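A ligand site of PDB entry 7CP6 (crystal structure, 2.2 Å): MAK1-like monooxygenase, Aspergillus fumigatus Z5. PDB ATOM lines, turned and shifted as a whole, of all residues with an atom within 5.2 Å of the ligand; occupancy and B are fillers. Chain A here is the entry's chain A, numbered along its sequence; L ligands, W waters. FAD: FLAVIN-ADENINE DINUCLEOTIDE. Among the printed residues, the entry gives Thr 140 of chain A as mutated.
O2B of the ligand is in hydrogen-bond range of OE2 of Glu 45 (2.5 Å).
N of Val 139 lies within hydrogen-bond range of N1A of the ligand, 3.0 Å away.
The backbone carbonyl oxygen (O) of Val 139 lies within hydrogen-bond range of a nitrogen (N6A) of the ligand, 2.7 Å away.
An oxygen (O4) of the ligand sits at hydrogen-bond distance from the backbone NH (N) of Val 59, at 3.0 Å.
The backbone carbonyl oxygen (O) of Val 59 is in hydrogen-bond range of a nitrogen (N3) of the ligand (2.8 Å).
The backbone NH of Asp 319 is in hydrogen-bond range of an oxygen (O2P) of the ligand (2.9 Å).
The side-chain carboxylate of Asp 319 is in hydrogen-bond range of an oxygen (O3') of the ligand, at 2.8 Å.
An oxygen (O1P) of the ligand lies within hydrogen-bond range of the backbone NH (N) of Gly 26 (3.0 Å).
NH2 of Arg 115 lies within hydrogen-bond range of O2' of the ligand (3.0 Å).
The backbone NH (N) of Gly 332 is in hydrogen-bond range of an oxygen (O2) of the ligand, at 3.0 Å.
O of Gly 331 sits close to O3' of the ligand.
The backbone NH (N) of Phe 25 lies within hydrogen-bond range of an oxygen (O1P) of the ligand (3.3 Å).
A nitrogen (N3A) of the ligand is in hydrogen-bond range of the backbone NH (N) of Lys 46, 3.4 Å away.
O of Glu 45 sits at hydrogen-bond distance from N of Ser 137 (2.8 Å).
OE1 of Glu 45 sits at hydrogen-bond distance from N of Leu 23 (2.6 Å).
N of Val 47 sits at hydrogen-bond distance from OE2 of Glu 45 (3.0 Å).
O of Leu 44 is in hydrogen-bond range of N of Gly 22 (2.7 Å).
O of Val 21 sits at hydrogen-bond distance from N of Ala 167 (2.9 Å).
O of Gly 169 lies close to N of Ala 320 (3.4 Å).
Residues that only touch the ligand: Val 21, Gly 22, Leu 23, Gly 24, Val 47, Ile 58, Ser 137, Arg 138, Ala 167, Asp 168, Gly 169, Asn 192, Leu 298, Gly 318, Pro 326, Gly 329 and Ser 333.
Hydrophobic or aromatic side chains that line the ligand: Val 21, Phe 25, Val 47, Ile 58, Val 59, Val 139, Leu 298 and Pro 326.
27 residues have an atom within 4 Å of the ligand: Val 21, Gly 22, Leu 23, Gly 24, Phe 25, Gly 26, Glu 45, Lys 46, Val 47, Ile 58, Val 59, Arg 115, Ser 137, Arg 138, Val 139, Ala 167, Asp 168, Gly 169, Asn 192, Leu 298, Gly 318, Asp 319, Pro 326, Gly 329, Gly 331, Gly 332 and Ser 333.
The nearest printed residue that does not touch the ligand is Gln 330 (4.01 Å).
Water W6 bridges an oxygen (O3B) of the ligand and the backbone carbonyl oxygen (O) of Leu 23.
Water W7 lies within hydrogen-bond range of the backbone carbonyl oxygen of Ala 167 (2.7 Å), an oxygen (O1P) of the ligand (2.7 Å), the backbone NH of Gly 27 (2.9 Å) and the backbone NH of Gly 24 (2.9 Å).
Water W1 lies within hydrogen-bond range of an oxygen (O1A) of the ligand (2.7 Å), the side-chain carboxylate (OD2) of Asp 319 (2.8 Å) and the backbone NH (N) of Val 170 (3.0 Å).
Water W5 bridges N7A of the ligand and OD2 of Asp 168.
Water W2 lies within hydrogen-bond range of OD2 of Asp 168 (2.6 Å) and N6A of the ligand (3.5 Å).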
ATOM      1  N   VAL A  21     -30.079  14.296  14.289  1.00  0.00           N
ATOM      2  CA  VAL A  21     -29.001  15.268  14.442  1.00  0.00           C
ATOM      3  C   VAL A  21     -28.910  15.641  15.906  1.00  0.00           C
ATOM      4  O   VAL A  21     -29.883  16.121  16.493  1.00  0.00           O
ATOM      5  CB  VAL A  21     -29.236  16.507  13.564  1.00  0.00           C
ATOM      6  CG1 VAL A  21     -28.047  17.461  13.688  1.00  0.00           C
ATOM      7  CG2 VAL A  21     -29.463  16.103  12.111  1.00  0.00           C
ATOM      8  N   GLY A  22     -27.734  15.430  16.502  1.00  0.00           N
ATOM      9  CA  GLY A  22     -27.481  15.831  17.872  1.00  0.00           C
ATOM     10  C   GLY A  22     -27.333  14.678  18.839  1.00  0.00           C
ATOM     11  O   GLY A  22     -28.157  13.755  18.839  1.00  0.00           O
ATOM     12  N   LEU A  23     -26.284  14.717  19.673  1.00  0.00           N
ATOM     13  CA  LEU A  23     -26.052  13.715  20.710  1.00  0.00           C
ATOM     14  C   LEU A  23     -26.482  14.210  22.093  1.00  0.00           C
ATOM     15  O   LEU A  23     -25.867  13.849  23.102  1.00  0.00           O
ATOM     16  CB  LEU A  23     -24.580  13.299  20.721  1.00  0.00           C
ATOM     17  CG  LEU A  23     -24.182  11.988  21.414  1.00  0.00           C
ATOM     18  CD1 LEU A  23     -24.772  10.783  20.706  1.00  0.00           C
ATOM     19  CD2 LEU A  23     -22.669  11.874  21.509  1.00  0.00           C
ATOM     20  N   GLY A  24     -27.514  15.039  22.146  1.00  0.00           N
ATOM     21  CA  GLY A  24     -28.082  15.489  23.407  1.00  0.00           C
ATOM     22  C   GLY A  24     -29.150  14.541  23.894  1.00  0.00           C
ATOM     23  O   GLY A  24     -29.207  13.368  23.499  1.00  0.00           O
ATOM     24  N   PHE A  25     -30.009  15.054  24.766  1.00  0.00           N
ATOM     25  CA  PHE A  25     -31.071  14.221  25.315  1.00  0.00           C
ATOM     26  C   PHE A  25     -32.141  13.928  24.268  1.00  0.00           C
ATOM     27  O   PHE A  25     -32.696  12.825  24.228  1.00  0.00           O
ATOM     28  CB  PHE A  25     -31.683  14.879  26.548  1.00  0.00           C
ATOM     29  CG  PHE A  25     -30.775  14.906  27.733  1.00  0.00           C
ATOM     30  CD1 PHE A  25     -30.569  13.757  28.490  1.00  0.00           C
ATOM     31  CD2 PHE A  25     -30.104  16.066  28.093  1.00  0.00           C
ATOM     32  CE1 PHE A  25     -29.720  13.780  29.577  1.00  0.00           C
ATOM     33  CE2 PHE A  25     -29.248  16.083  29.174  1.00  0.00           C
ATOM     34  CZ  PHE A  25     -29.056  14.942  29.925  1.00  0.00           C
ATOM     35  N   GLY A  26     -32.441  14.895  23.401  1.00  0.00           N
ATOM     36  CA  GLY A  26     -33.417  14.663  22.354  1.00  0.00           C
ATOM     37  C   GLY A  26     -32.903  13.691  21.296  1.00  0.00           C
ATOM     38  O   GLY A  26     -33.610  12.764  20.890  1.00  0.00           O
ATOM     39  N   GLY A  27     -31.669  13.901  20.846  1.00  0.00           N
ATOM     40  CA  GLY A  27     -31.136  13.076  19.772  1.00  0.00           C
ATOM     41  C   GLY A  27     -30.885  11.645  20.196  1.00  0.00           C
ATOM     42  O   GLY A  27     -31.239  10.700  19.480  1.00  0.00           O
ATOM     43  N   LEU A  44     -26.096  11.879  13.848  1.00  0.00           N
ATOM     44  CA  LEU A  44     -24.999  12.760  13.476  1.00  0.00           C
ATOM     45  C   LEU A  44     -24.753  13.768  14.584  1.00  0.00           C
ATOM     46  O   LEU A  44     -25.681  14.442  15.036  1.00  0.00           O
ATOM     47  CB  LEU A  44     -25.298  13.477  12.156  1.00  0.00           C
ATOM     48  CG  LEU A  44     -25.600  12.562  10.970  1.00  0.00           C
ATOM     49  CD1 LEU A  44     -26.154  13.358   9.800  1.00  0.00           C
ATOM     50  CD2 LEU A  44     -24.348  11.796  10.558  1.00  0.00           C
ATOM     51  N   GLU A  45     -23.493  13.868  15.029  1.00  0.00           N
ATOM     52  CA  GLU A  45     -23.102  14.789  16.087  1.00  0.00           C
ATOM     53  C   GLU A  45     -21.780  15.441  15.712  1.00  0.00           C
ATOM     54  O   GLU A  45     -20.874  14.768  15.207  1.00  0.00           O
ATOM     55  CB  GLU A  45     -22.987  14.075  17.436  1.00  0.00           C
ATOM     56  CG  GLU A  45     -22.239  14.859  18.506  1.00  0.00           C
ATOM     57  CD  GLU A  45     -22.950  16.143  18.902  1.00  0.00           C
ATOM     58  OE1 GLU A  45     -24.162  16.084  19.192  1.00  0.00           O
ATOM     59  OE2 GLU A  45     -22.298  17.204  18.918  1.00  0.00           O
ATOM     60  N   LYS A  46     -21.673  16.751  15.961  1.00  0.00           N
ATOM     61  CA  LYS A  46     -20.491  17.492  15.517  1.00  0.00           C
ATOM     62  C   LYS A  46     -19.292  17.301  16.428  1.00  0.00           C
ATOM     63  O   LYS A  46     -18.150  17.314  15.949  1.00  0.00           O
ATOM     64  CB  LYS A  46     -20.825  18.979  15.386  1.00  0.00           C
ATOM     65  CG  LYS A  46     -21.230  19.658  16.679  1.00  0.00           C
ATOM     66  CD  LYS A  46     -21.539  21.129  16.438  1.00  0.00           C
ATOM     67  CE  LYS A  46     -21.900  21.841  17.734  1.00  0.00           C
ATOM     68  NZ  LYS A  46     -22.239  23.275  17.514  1.00  0.00           N
ATOM     69  N   VAL A  47     -19.499  17.115  17.738  1.00  0.00           N
ATOM     70  CA  VAL A  47     -18.371  16.951  18.645  1.00  0.00           C
ATOM     71  C   VAL A  47     -17.750  15.571  18.458  1.00  0.00           C
ATOM     72  O   VAL A  47     -18.424  14.610  18.035  1.00  0.00           O
ATOM     73  CB  VAL A  47     -18.793  17.187  20.104  1.00  0.00           C
ATOM     74  CG1 VAL A  47     -19.487  18.533  20.247  1.00  0.00           C
ATOM     75  CG2 VAL A  47     -19.676  16.056  20.603  1.00  0.00           C
ATOM     76  N   ALA A  57     -24.453  19.885  36.820  1.00  0.00           N
ATOM     77  CA  ALA A  57     -25.449  19.050  37.463  1.00  0.00           C
ATOM     78  C   ALA A  57     -26.828  19.309  36.881  1.00  0.00           C
ATOM     79  O   ALA A  57     -27.180  20.442  36.552  1.00  0.00           O
ATOM     80  CB  ALA A  57     -25.466  19.324  38.971  1.00  0.00           C
ATOM     81  N   ILE A  58     -27.611  18.245  36.727  1.00  0.00           N
ATOM     82  CA  ILE A  58     -28.940  18.316  36.139  1.00  0.00           C
ATOM     83  C   ILE A  58     -29.887  17.395  36.906  1.00  0.00           C
ATOM     84  O   ILE A  58     -29.465  16.422  37.540  1.00  0.00           O
ATOM     85  CB  ILE A  58     -28.940  17.961  34.638  1.00  0.00           C
ATOM     86  CG1 ILE A  58     -28.098  16.704  34.374  1.00  0.00           C
ATOM     87  CG2 ILE A  58     -28.426  19.121  33.801  1.00  0.00           C
ATOM     88  CD1 ILE A  58     -28.900  15.417  34.343  1.00  0.00           C
ATOM     89  N   VAL A  59     -31.173  17.719  36.827  1.00  0.00           N
ATOM     90  CA  VAL A  59     -32.224  16.924  37.451  1.00  0.00           C
ATOM     91  C   VAL A  59     -33.079  16.328  36.347  1.00  0.00           C
ATOM     92  O   VAL A  59     -33.600  17.059  35.482  1.00  0.00           O
ATOM     93  CB  VAL A  59     -33.078  17.769  38.407  1.00  0.00           C
ATOM     94  CG1 VAL A  59     -34.231  16.945  38.964  1.00  0.00           C
ATOM     95  CG2 VAL A  59     -32.223  18.315  39.546  1.00  0.00           C
ATOM     96  N   ILE A  60     -33.230  15.006  36.356  1.00  0.00           N
ATOM     97  CA  ILE A  60     -34.085  14.298  35.420  1.00  0.00           C
ATOM     98  C   ILE A  60     -35.334  13.849  36.179  1.00  0.00           C
ATOM     99  O   ILE A  60     -35.226  13.151  37.192  1.00  0.00           O
ATOM    100  CB  ILE A  60     -33.363  13.094  34.787  1.00  0.00           C
ATOM    101  CG1 ILE A  60     -32.092  13.555  34.065  1.00  0.00           C
ATOM    102  CG2 ILE A  60     -34.283  12.368  33.821  1.00  0.00           C
ATOM    103  CD1 ILE A  60     -32.350  14.502  32.911  1.00  0.00           C
ATOM    104  N   ARG A 115     -24.488  15.793  33.953  1.00  0.00           N
ATOM    105  CA  ARG A 115     -24.970  15.733  32.579  1.00  0.00           C
ATOM    106  C   ARG A 115     -24.081  14.859  31.705  1.00  0.00           C
ATOM    107  O   ARG A 115     -24.540  13.881  31.107  1.00  0.00           O
ATOM    108  CB  ARG A 115     -25.071  17.148  31.994  1.00  0.00           C
ATOM    109  CG  ARG A 115     -25.377  17.169  30.507  1.00  0.00           C
ATOM    110  CD  ARG A 115     -25.146  18.551  29.907  1.00  0.00           C
ATOM    111  NE  ARG A 115     -25.929  19.576  30.594  1.00  0.00           N
ATOM    112  CZ  ARG A 115     -27.179  19.897  30.284  1.00  0.00           C
ATOM    113  NH1 ARG A 115     -27.798  19.273  29.291  1.00  0.00           N
ATOM    114  NH2 ARG A 115     -27.816  20.840  30.980  1.00  0.00           N
ATOM    115  N   SER A 137     -19.375  14.985  12.911  1.00  0.00           N
ATOM    116  CA  SER A 137     -20.199  15.149  11.710  1.00  0.00           C
ATOM    117  C   SER A 137     -21.029  16.417  11.876  1.00  0.00           C
ATOM    118  O   SER A 137     -22.127  16.380  12.441  1.00  0.00           O
ATOM    119  CB  SER A 137     -21.082  13.917  11.485  1.00  0.00           C
ATOM    120  OG  SER A 137     -20.303  12.739  11.413  1.00  0.00           O
ATOM    121  N   ARG A 138     -20.508  17.537  11.379  1.00  0.00           N
ATOM    122  CA  ARG A 138     -21.249  18.798  11.431  1.00  0.00           C
ATOM    123  C   ARG A 138     -22.323  18.817  10.354  1.00  0.00           C
ATOM    124  O   ARG A 138     -22.042  18.571   9.181  1.00  0.00           O
ATOM    125  CB  ARG A 138     -20.300  19.992  11.259  1.00  0.00           C
ATOM    126  CG  ARG A 138     -20.872  21.290  11.789  1.00  0.00           C
ATOM    127  CD  ARG A 138     -20.180  22.508  11.193  1.00  0.00           C
ATOM    128  NE  ARG A 138     -20.541  22.714   9.790  1.00  0.00           N
ATOM    129  CZ  ARG A 138     -19.741  22.431   8.762  1.00  0.00           C
ATOM    130  NH1 ARG A 138     -18.521  21.956   8.960  1.00  0.00           N
ATOM    131  NH2 ARG A 138     -20.169  22.650   7.518  1.00  0.00           N
ATOM    132  N   VAL A 139     -23.548  19.112  10.760  1.00  0.00           N
ATOM    133  CA  VAL A 139     -24.711  19.089   9.873  1.00  0.00           C
ATOM    134  C   VAL A 139     -25.090  20.509   9.492  1.00  0.00           C
ATOM    135  O   VAL A 139     -25.094  21.416  10.347  1.00  0.00           O
ATOM    136  CB  VAL A 139     -25.894  18.356  10.553  1.00  0.00           C
ATOM    137  CG1 VAL A 139     -27.161  18.538   9.741  1.00  0.00           C
ATOM    138  CG2 VAL A 139     -25.572  16.887  10.727  1.00  0.00           C
ATOM    139  N   THR A 140     -25.405  20.709   8.219  1.00  0.00           N
ATOM    140  CA  THR A 140     -25.976  21.961   7.741  1.00  0.00           C
ATOM    141  C   THR A 140     -26.607  21.696   6.370  1.00  0.00           C
ATOM    142  O   THR A 140     -26.573  20.573   5.860  1.00  0.00           O
ATOM    143  CB  THR A 140     -24.927  23.083   7.665  1.00  0.00           C
ATOM    144  OG1 THR A 140     -25.493  24.216   6.999  1.00  0.00           O
ATOM    145  CG2 THR A 140     -23.710  22.606   6.921  1.00  0.00           C
ATOM    146  N   ALA A 167     -32.430  17.549  16.578  1.00  0.00           N
ATOM    147  CA  ALA A 167     -32.306  17.863  17.989  1.00  0.00           C
ATOM    148  C   ALA A 167     -30.967  18.544  18.259  1.00  0.00           C
ATOM    149  O   ALA A 167     -30.176  18.076  19.079  1.00  0.00           O
ATOM    150  CB  ALA A 167     -32.441  16.595  18.839  1.00  0.00           C
ATOM    151  N   ASP A 168     -30.706  19.651  17.560  1.00  0.00           N
ATOM    152  CA  ASP A 168     -29.402  20.310  17.581  1.00  0.00           C
ATOM    153  C   ASP A 168     -29.323  21.472  18.571  1.00  0.00           C
ATOM    154  O   ASP A 168     -28.420  22.307  18.452  1.00  0.00           O
ATOM    155  CB  ASP A 168     -29.039  20.774  16.173  1.00  0.00           C
ATOM    156  CG  ASP A 168     -30.131  21.595  15.519  1.00  0.00           C
ATOM    157  OD1 ASP A 168     -31.291  21.499  15.964  1.00  0.00           O
ATOM    158  OD2 ASP A 168     -29.833  22.330  14.554  1.00  0.00           O
ATOM    159  N   GLY A 169     -30.245  21.547  19.520  1.00  0.00           N
ATOM    160  CA  GLY A 169     -30.100  22.489  20.622  1.00  0.00           C
ATOM    161  C   GLY A 169     -30.690  23.857  20.355  1.00  0.00           C
ATOM    162  O   GLY A 169     -31.315  24.127  19.330  1.00  0.00           O
ATOM    163  N   VAL A 170     -30.444  24.753  21.322  1.00  0.00           N
ATOM    164  CA  VAL A 170     -31.029  26.101  21.266  1.00  0.00           C
ATOM    165  C   VAL A 170     -30.510  26.874  20.054  1.00  0.00           C
ATOM    166  O   VAL A 170     -31.250  27.622  19.417  1.00  0.00           O
ATOM    167  CB  VAL A 170     -30.751  26.858  22.578  1.00  0.00           C
ATOM    168  CG1 VAL A 170     -31.626  26.329  23.698  1.00  0.00           C
ATOM    169  CG2 VAL A 170     -29.287  26.759  22.955  1.00  0.00           C
ATOM    170  N   ASN A 192     -25.634  32.778  32.006  1.00  0.00           N
ATOM    171  CA  ASN A 192     -25.533  31.826  33.113  1.00  0.00           C
ATOM    172  C   ASN A 192     -24.071  31.524  33.388  1.00  0.00           C
ATOM    173  O   ASN A 192     -23.406  30.867  32.574  1.00  0.00           O
ATOM    174  CB  ASN A 192     -26.299  30.541  32.802  1.00  0.00           C
ATOM    175  CG  ASN A 192     -26.248  29.541  33.934  1.00  0.00           C
ATOM    176  OD1 ASN A 192     -26.874  29.727  34.984  1.00  0.00           O
ATOM    177  ND2 ASN A 192     -25.498  28.460  33.734  1.00  0.00           N
ATOM    178  N   LEU A 298     -27.927  32.788  27.500  1.00  0.00           N
ATOM    179  CA  LEU A 298     -29.131  31.966  27.454  1.00  0.00           C
ATOM    180  C   LEU A 298     -30.022  32.413  26.292  1.00  0.00           C
ATOM    181  O   LEU A 298     -30.145  33.601  26.014  1.00  0.00           O
ATOM    182  CB  LEU A 298     -29.901  32.062  28.772  1.00  0.00           C
ATOM    183  CG  LEU A 298     -29.152  31.553  30.013  1.00  0.00           C
ATOM    184  CD1 LEU A 298     -29.929  31.888  31.277  1.00  0.00           C
ATOM    185  CD2 LEU A 298     -28.901  30.054  29.918  1.00  0.00           C
ATOM    186  N   ILE A 317     -37.180  18.930  17.469  1.00  0.00           N
ATOM    187  CA  ILE A 317     -37.530  18.467  18.812  1.00  0.00           C
ATOM    188  C   ILE A 317     -36.536  19.083  19.800  1.00  0.00           C
ATOM    189  O   ILE A 317     -35.535  19.672  19.420  1.00  0.00           O
ATOM    190  CB  ILE A 317     -37.523  16.929  18.936  1.00  0.00           C
ATOM    191  CG1 ILE A 317     -36.110  16.377  18.730  1.00  0.00           C
ATOM    192  CG2 ILE A 317     -38.503  16.299  17.962  1.00  0.00           C
ATOM    193  CD1 ILE A 317     -35.975  14.896  19.068  1.00  0.00           C
ATOM    194  N   GLY A 318     -36.856  18.922  21.091  1.00  0.00           N
ATOM    195  CA  GLY A 318     -35.951  19.377  22.137  1.00  0.00           C
ATOM    196  C   GLY A 318     -35.841  20.889  22.205  1.00  0.00           C
ATOM    197  O   GLY A 318     -36.785  21.632  21.925  1.00  0.00           O
ATOM    198  N   ASP A 319     -34.640  21.360  22.580  1.00  0.00           N
ATOM    199  CA  ASP A 319     -34.390  22.796  22.701  1.00  0.00           C
ATOM    200  C   ASP A 319     -34.548  23.515  21.370  1.00  0.00           C
ATOM    201  O   ASP A 319     -34.876  24.699  21.343  1.00  0.00           O
ATOM    202  CB  ASP A 319     -32.994  23.045  23.268  1.00  0.00           C
ATOM    203  CG  ASP A 319     -32.972  23.020  24.778  1.00  0.00           C
ATOM    204  OD1 ASP A 319     -34.007  22.708  25.392  1.00  0.00           O
ATOM    205  OD2 ASP A 319     -31.893  23.309  25.352  1.00  0.00           O
ATOM    206  N   ALA A 320     -34.295  22.815  20.259  1.00  0.00           N
ATOM    207  CA  ALA A 320     -34.470  23.428  18.941  1.00  0.00           C
ATOM    208  C   ALA A 320     -35.905  23.869  18.711  1.00  0.00           C
ATOM    209  O   ALA A 320     -36.144  24.851  17.992  1.00  0.00           O
ATOM    210  CB  ALA A 320     -34.021  22.456  17.856  1.00  0.00           C
ATOM    211  N   PRO A 326     -34.398  27.959  32.577  1.00  0.00           N
ATOM    212  CA  PRO A 326     -33.974  26.868  33.468  1.00  0.00           C
ATOM    213  C   PRO A 326     -34.470  27.024  34.894  1.00  0.00           C
ATOM    214  O   PRO A 326     -33.668  27.254  35.805  1.00  0.00           O
ATOM    215  CB  PRO A 326     -32.437  26.941  33.407  1.00  0.00           C
ATOM    216  CG  PRO A 326     -32.118  27.816  32.232  1.00  0.00           C
ATOM    217  CD  PRO A 326     -33.256  28.773  32.117  1.00  0.00           C
ATOM    218  N   GLY A 329     -36.817  22.514  35.510  1.00  0.00           N
ATOM    219  CA  GLY A 329     -36.201  21.200  35.610  1.00  0.00           C
ATOM    220  C   GLY A 329     -36.811  20.164  34.704  1.00  0.00           C
ATOM    221  O   GLY A 329     -36.892  18.984  35.082  1.00  0.00           O
ATOM    222  N   GLN A 330     -37.253  20.558  33.510  1.00  0.00           N
ATOM    223  CA  GLN A 330     -37.915  19.641  32.602  1.00  0.00           C
ATOM    224  C   GLN A 330     -37.446  19.739  31.161  1.00  0.00           C
ATOM    225  O   GLN A 330     -38.014  19.064  30.296  1.00  0.00           O
ATOM    226  CB  GLN A 330     -39.436  19.861  32.644  1.00  0.00           C
ATOM    227  CG  GLN A 330     -40.128  19.219  33.837  1.00  0.00           C
ATOM    228  CD  GLN A 330     -40.275  17.718  33.685  1.00  0.00           C
ATOM    229  OE1 GLN A 330     -40.652  17.222  32.620  1.00  0.00           O
ATOM    230  NE2 GLN A 330     -39.969  16.984  34.748  1.00  0.00           N
ATOM    231  N   GLY A 331     -36.420  20.549  30.872  1.00  0.00           N
ATOM    232  CA  GLY A 331     -35.976  20.687  29.493  1.00  0.00           C
ATOM    233  C   GLY A 331     -35.476  19.387  28.907  1.00  0.00           C
ATOM    234  O   GLY A 331     -35.843  18.994  27.800  1.00  0.00           O
ATOM    235  N   GLY A 332     -34.625  18.675  29.657  1.00  0.00           N
ATOM    236  CA  GLY A 332     -34.129  17.397  29.185  1.00  0.00           C
ATOM    237  C   GLY A 332     -35.206  16.329  29.160  1.00  0.00           C
ATOM    238  O   GLY A 332     -35.264  15.513  28.240  1.00  0.00           O
ATOM    239  N   SER A 333     -36.094  16.327  30.162  1.00  0.00           N
ATOM    240  CA  SER A 333     -37.167  15.343  30.213  1.00  0.00           C
ATOM    241  C   SER A 333     -38.131  15.520  29.049  1.00  0.00           C
ATOM    242  O   SER A 333     -38.611  14.534  28.471  1.00  0.00           O
ATOM    243  CB  SER A 333     -37.916  15.426  31.534  1.00  0.00           C
ATOM    244  OG  SER A 333     -37.073  15.066  32.612  1.00  0.00           O
ATOM    245  N   ALA A 335     -37.344  16.882  26.138  1.00  0.00           N
ATOM    246  CA  ALA A 335     -36.632  16.442  24.940  1.00  0.00           C
ATOM    247  C   ALA A 335     -36.673  14.923  24.813  1.00  0.00           C
ATOM    248  O   ALA A 335     -36.740  14.398  23.696  1.00  0.00           O
ATOM    249  CB  ALA A 335     -35.191  16.945  24.957  1.00  0.00           C
HETATM  250  PA  FAD L   1     -28.704  19.628  23.477  1.00  0.00           P
HETATM  251  O1A FAD L   1     -28.239  20.931  23.574  1.00  0.00           O
HETATM  252  O2A FAD L   1     -28.517  18.867  24.609  1.00  0.00           O
HETATM  253  O5B FAD L   1     -28.021  18.927  22.287  1.00  0.00           O
HETATM  254  C5B FAD L   1     -27.667  19.447  21.049  1.00  0.00           C
HETATM  255  C4B FAD L   1     -26.615  18.601  20.389  1.00  0.00           C
HETATM  256  O4B FAD L   1     -26.549  18.844  19.023  1.00  0.00           O
HETATM  257  C3B FAD L   1     -25.235  18.849  20.915  1.00  0.00           C
HETATM  258  O3B FAD L   1     -24.672  17.634  21.279  1.00  0.00           O
HETATM  259  C2B FAD L   1     -24.543  19.585  19.819  1.00  0.00           C
HETATM  260  O2B FAD L   1     -23.187  19.301  19.827  1.00  0.00           O
HETATM  261  C1B FAD L   1     -25.243  19.060  18.605  1.00  0.00           C
HETATM  262  N9A FAD L   1     -25.243  19.923  17.432  1.00  0.00           N
HETATM  263  C8A FAD L   1     -25.527  21.174  17.370  1.00  0.00           C
HETATM  264  N7A FAD L   1     -25.437  21.609  16.149  1.00  0.00           N
HETATM  265  C5A FAD L   1     -25.108  20.615  15.392  1.00  0.00           C
HETATM  266  C6A FAD L   1     -24.841  20.357  13.967  1.00  0.00           C
HETATM  267  N6A FAD L   1     -24.922  21.318  13.082  1.00  0.00           N
HETATM  268  N1A FAD L   1     -24.523  19.143  13.605  1.00  0.00           N
HETATM  269  C2A FAD L   1     -24.420  18.224  14.473  1.00  0.00           C
HETATM  270  N3A FAD L   1     -24.644  18.375  15.750  1.00  0.00           N
HETATM  271  C4A FAD L   1     -24.982  19.520  16.265  1.00  0.00           C
HETATM  272  N1  FAD L   1     -32.900  20.224  31.997  1.00  0.00           N
HETATM  273  C2  FAD L   1     -33.256  19.308  32.880  1.00  0.00           C
HETATM  274  O2  FAD L   1     -33.940  18.384  32.544  1.00  0.00           O
HETATM  275  N3  FAD L   1     -32.875  19.387  34.135  1.00  0.00           N
HETATM  276  C4  FAD L   1     -32.116  20.342  34.581  1.00  0.00           C
HETATM  277  O4  FAD L   1     -31.781  20.406  35.728  1.00  0.00           O
HETATM  278  C4X FAD L   1     -31.686  21.368  33.676  1.00  0.00           C
HETATM  279  N5  FAD L   1     -30.913  22.376  34.061  1.00  0.00           N
HETATM  280  C5X FAD L   1     -30.536  23.296  33.183  1.00  0.00           C
HETATM  281  C6  FAD L   1     -29.761  24.346  33.565  1.00  0.00           C
HETATM  282  C7  FAD L   1     -29.370  25.285  32.663  1.00  0.00           C
HETATM  283  C7M FAD L   1     -28.528  26.434  33.068  1.00  0.00           C
HETATM  284  C8  FAD L   1     -29.804  25.193  31.288  1.00  0.00           C
HETATM  285  C8M FAD L   1     -29.369  26.215  30.313  1.00  0.00           C
HETATM  286  C9  FAD L   1     -30.571  24.169  30.889  1.00  0.00           C
HETATM  287  C9A FAD L   1     -30.977  23.213  31.789  1.00  0.00           C
HETATM  288  N10 FAD L   1     -31.788  22.149  31.393  1.00  0.00           N
HETATM  289  C10 FAD L   1     -32.164  21.230  32.313  1.00  0.00           C
HETATM  290  C1' FAD L   1     -32.243  22.019  30.052  1.00  0.00           C
HETATM  291  C2' FAD L   1     -31.492  21.005  29.226  1.00  0.00           C
HETATM  292  O2' FAD L   1     -30.203  21.410  29.288  1.00  0.00           O
HETATM  293  C3' FAD L   1     -31.924  21.008  27.789  1.00  0.00           C
HETATM  294  O3' FAD L   1     -33.271  21.225  27.707  1.00  0.00           O
HETATM  295  C4' FAD L   1     -31.654  19.726  27.029  1.00  0.00           C
HETATM  296  O4' FAD L   1     -30.288  19.473  27.118  1.00  0.00           O
HETATM  297  C5' FAD L   1     -32.119  19.828  25.599  1.00  0.00           C
HETATM  298  O5' FAD L   1     -31.578  18.829  24.813  1.00  0.00           O
HETATM  299  P   FAD L   1     -31.410  18.822  23.316  1.00  0.00           P
HETATM  300  O1P FAD L   1     -31.173  17.540  22.960  1.00  0.00           O
HETATM  301  O2P FAD L   1     -32.530  19.344  22.838  1.00  0.00           O
HETATM  302  O3P FAD L   1     -30.185  19.714  23.008  1.00  0.00           O
HETATM  303  O   HOH W   1     -29.560  23.325  23.821  1.00  0.00           O
HETATM  304  O   HOH W   2     -28.335  21.654  12.585  1.00  0.00           O
HETATM  305  O   HOH W   3     -32.912  20.260  20.178  1.00  0.00           O
HETATM  306  O   HOH W   4     -35.996  17.092  33.604  1.00  0.00           O
HETATM  307  O   HOH W   5     -26.971  23.939  15.007  1.00  0.00           O
HETATM  308  O   HOH W   6     -24.253  16.290  23.449  1.00  0.00           O
HETATM  309  O   HOH W   7     -29.918  16.193  20.938  1.00  0.00           O
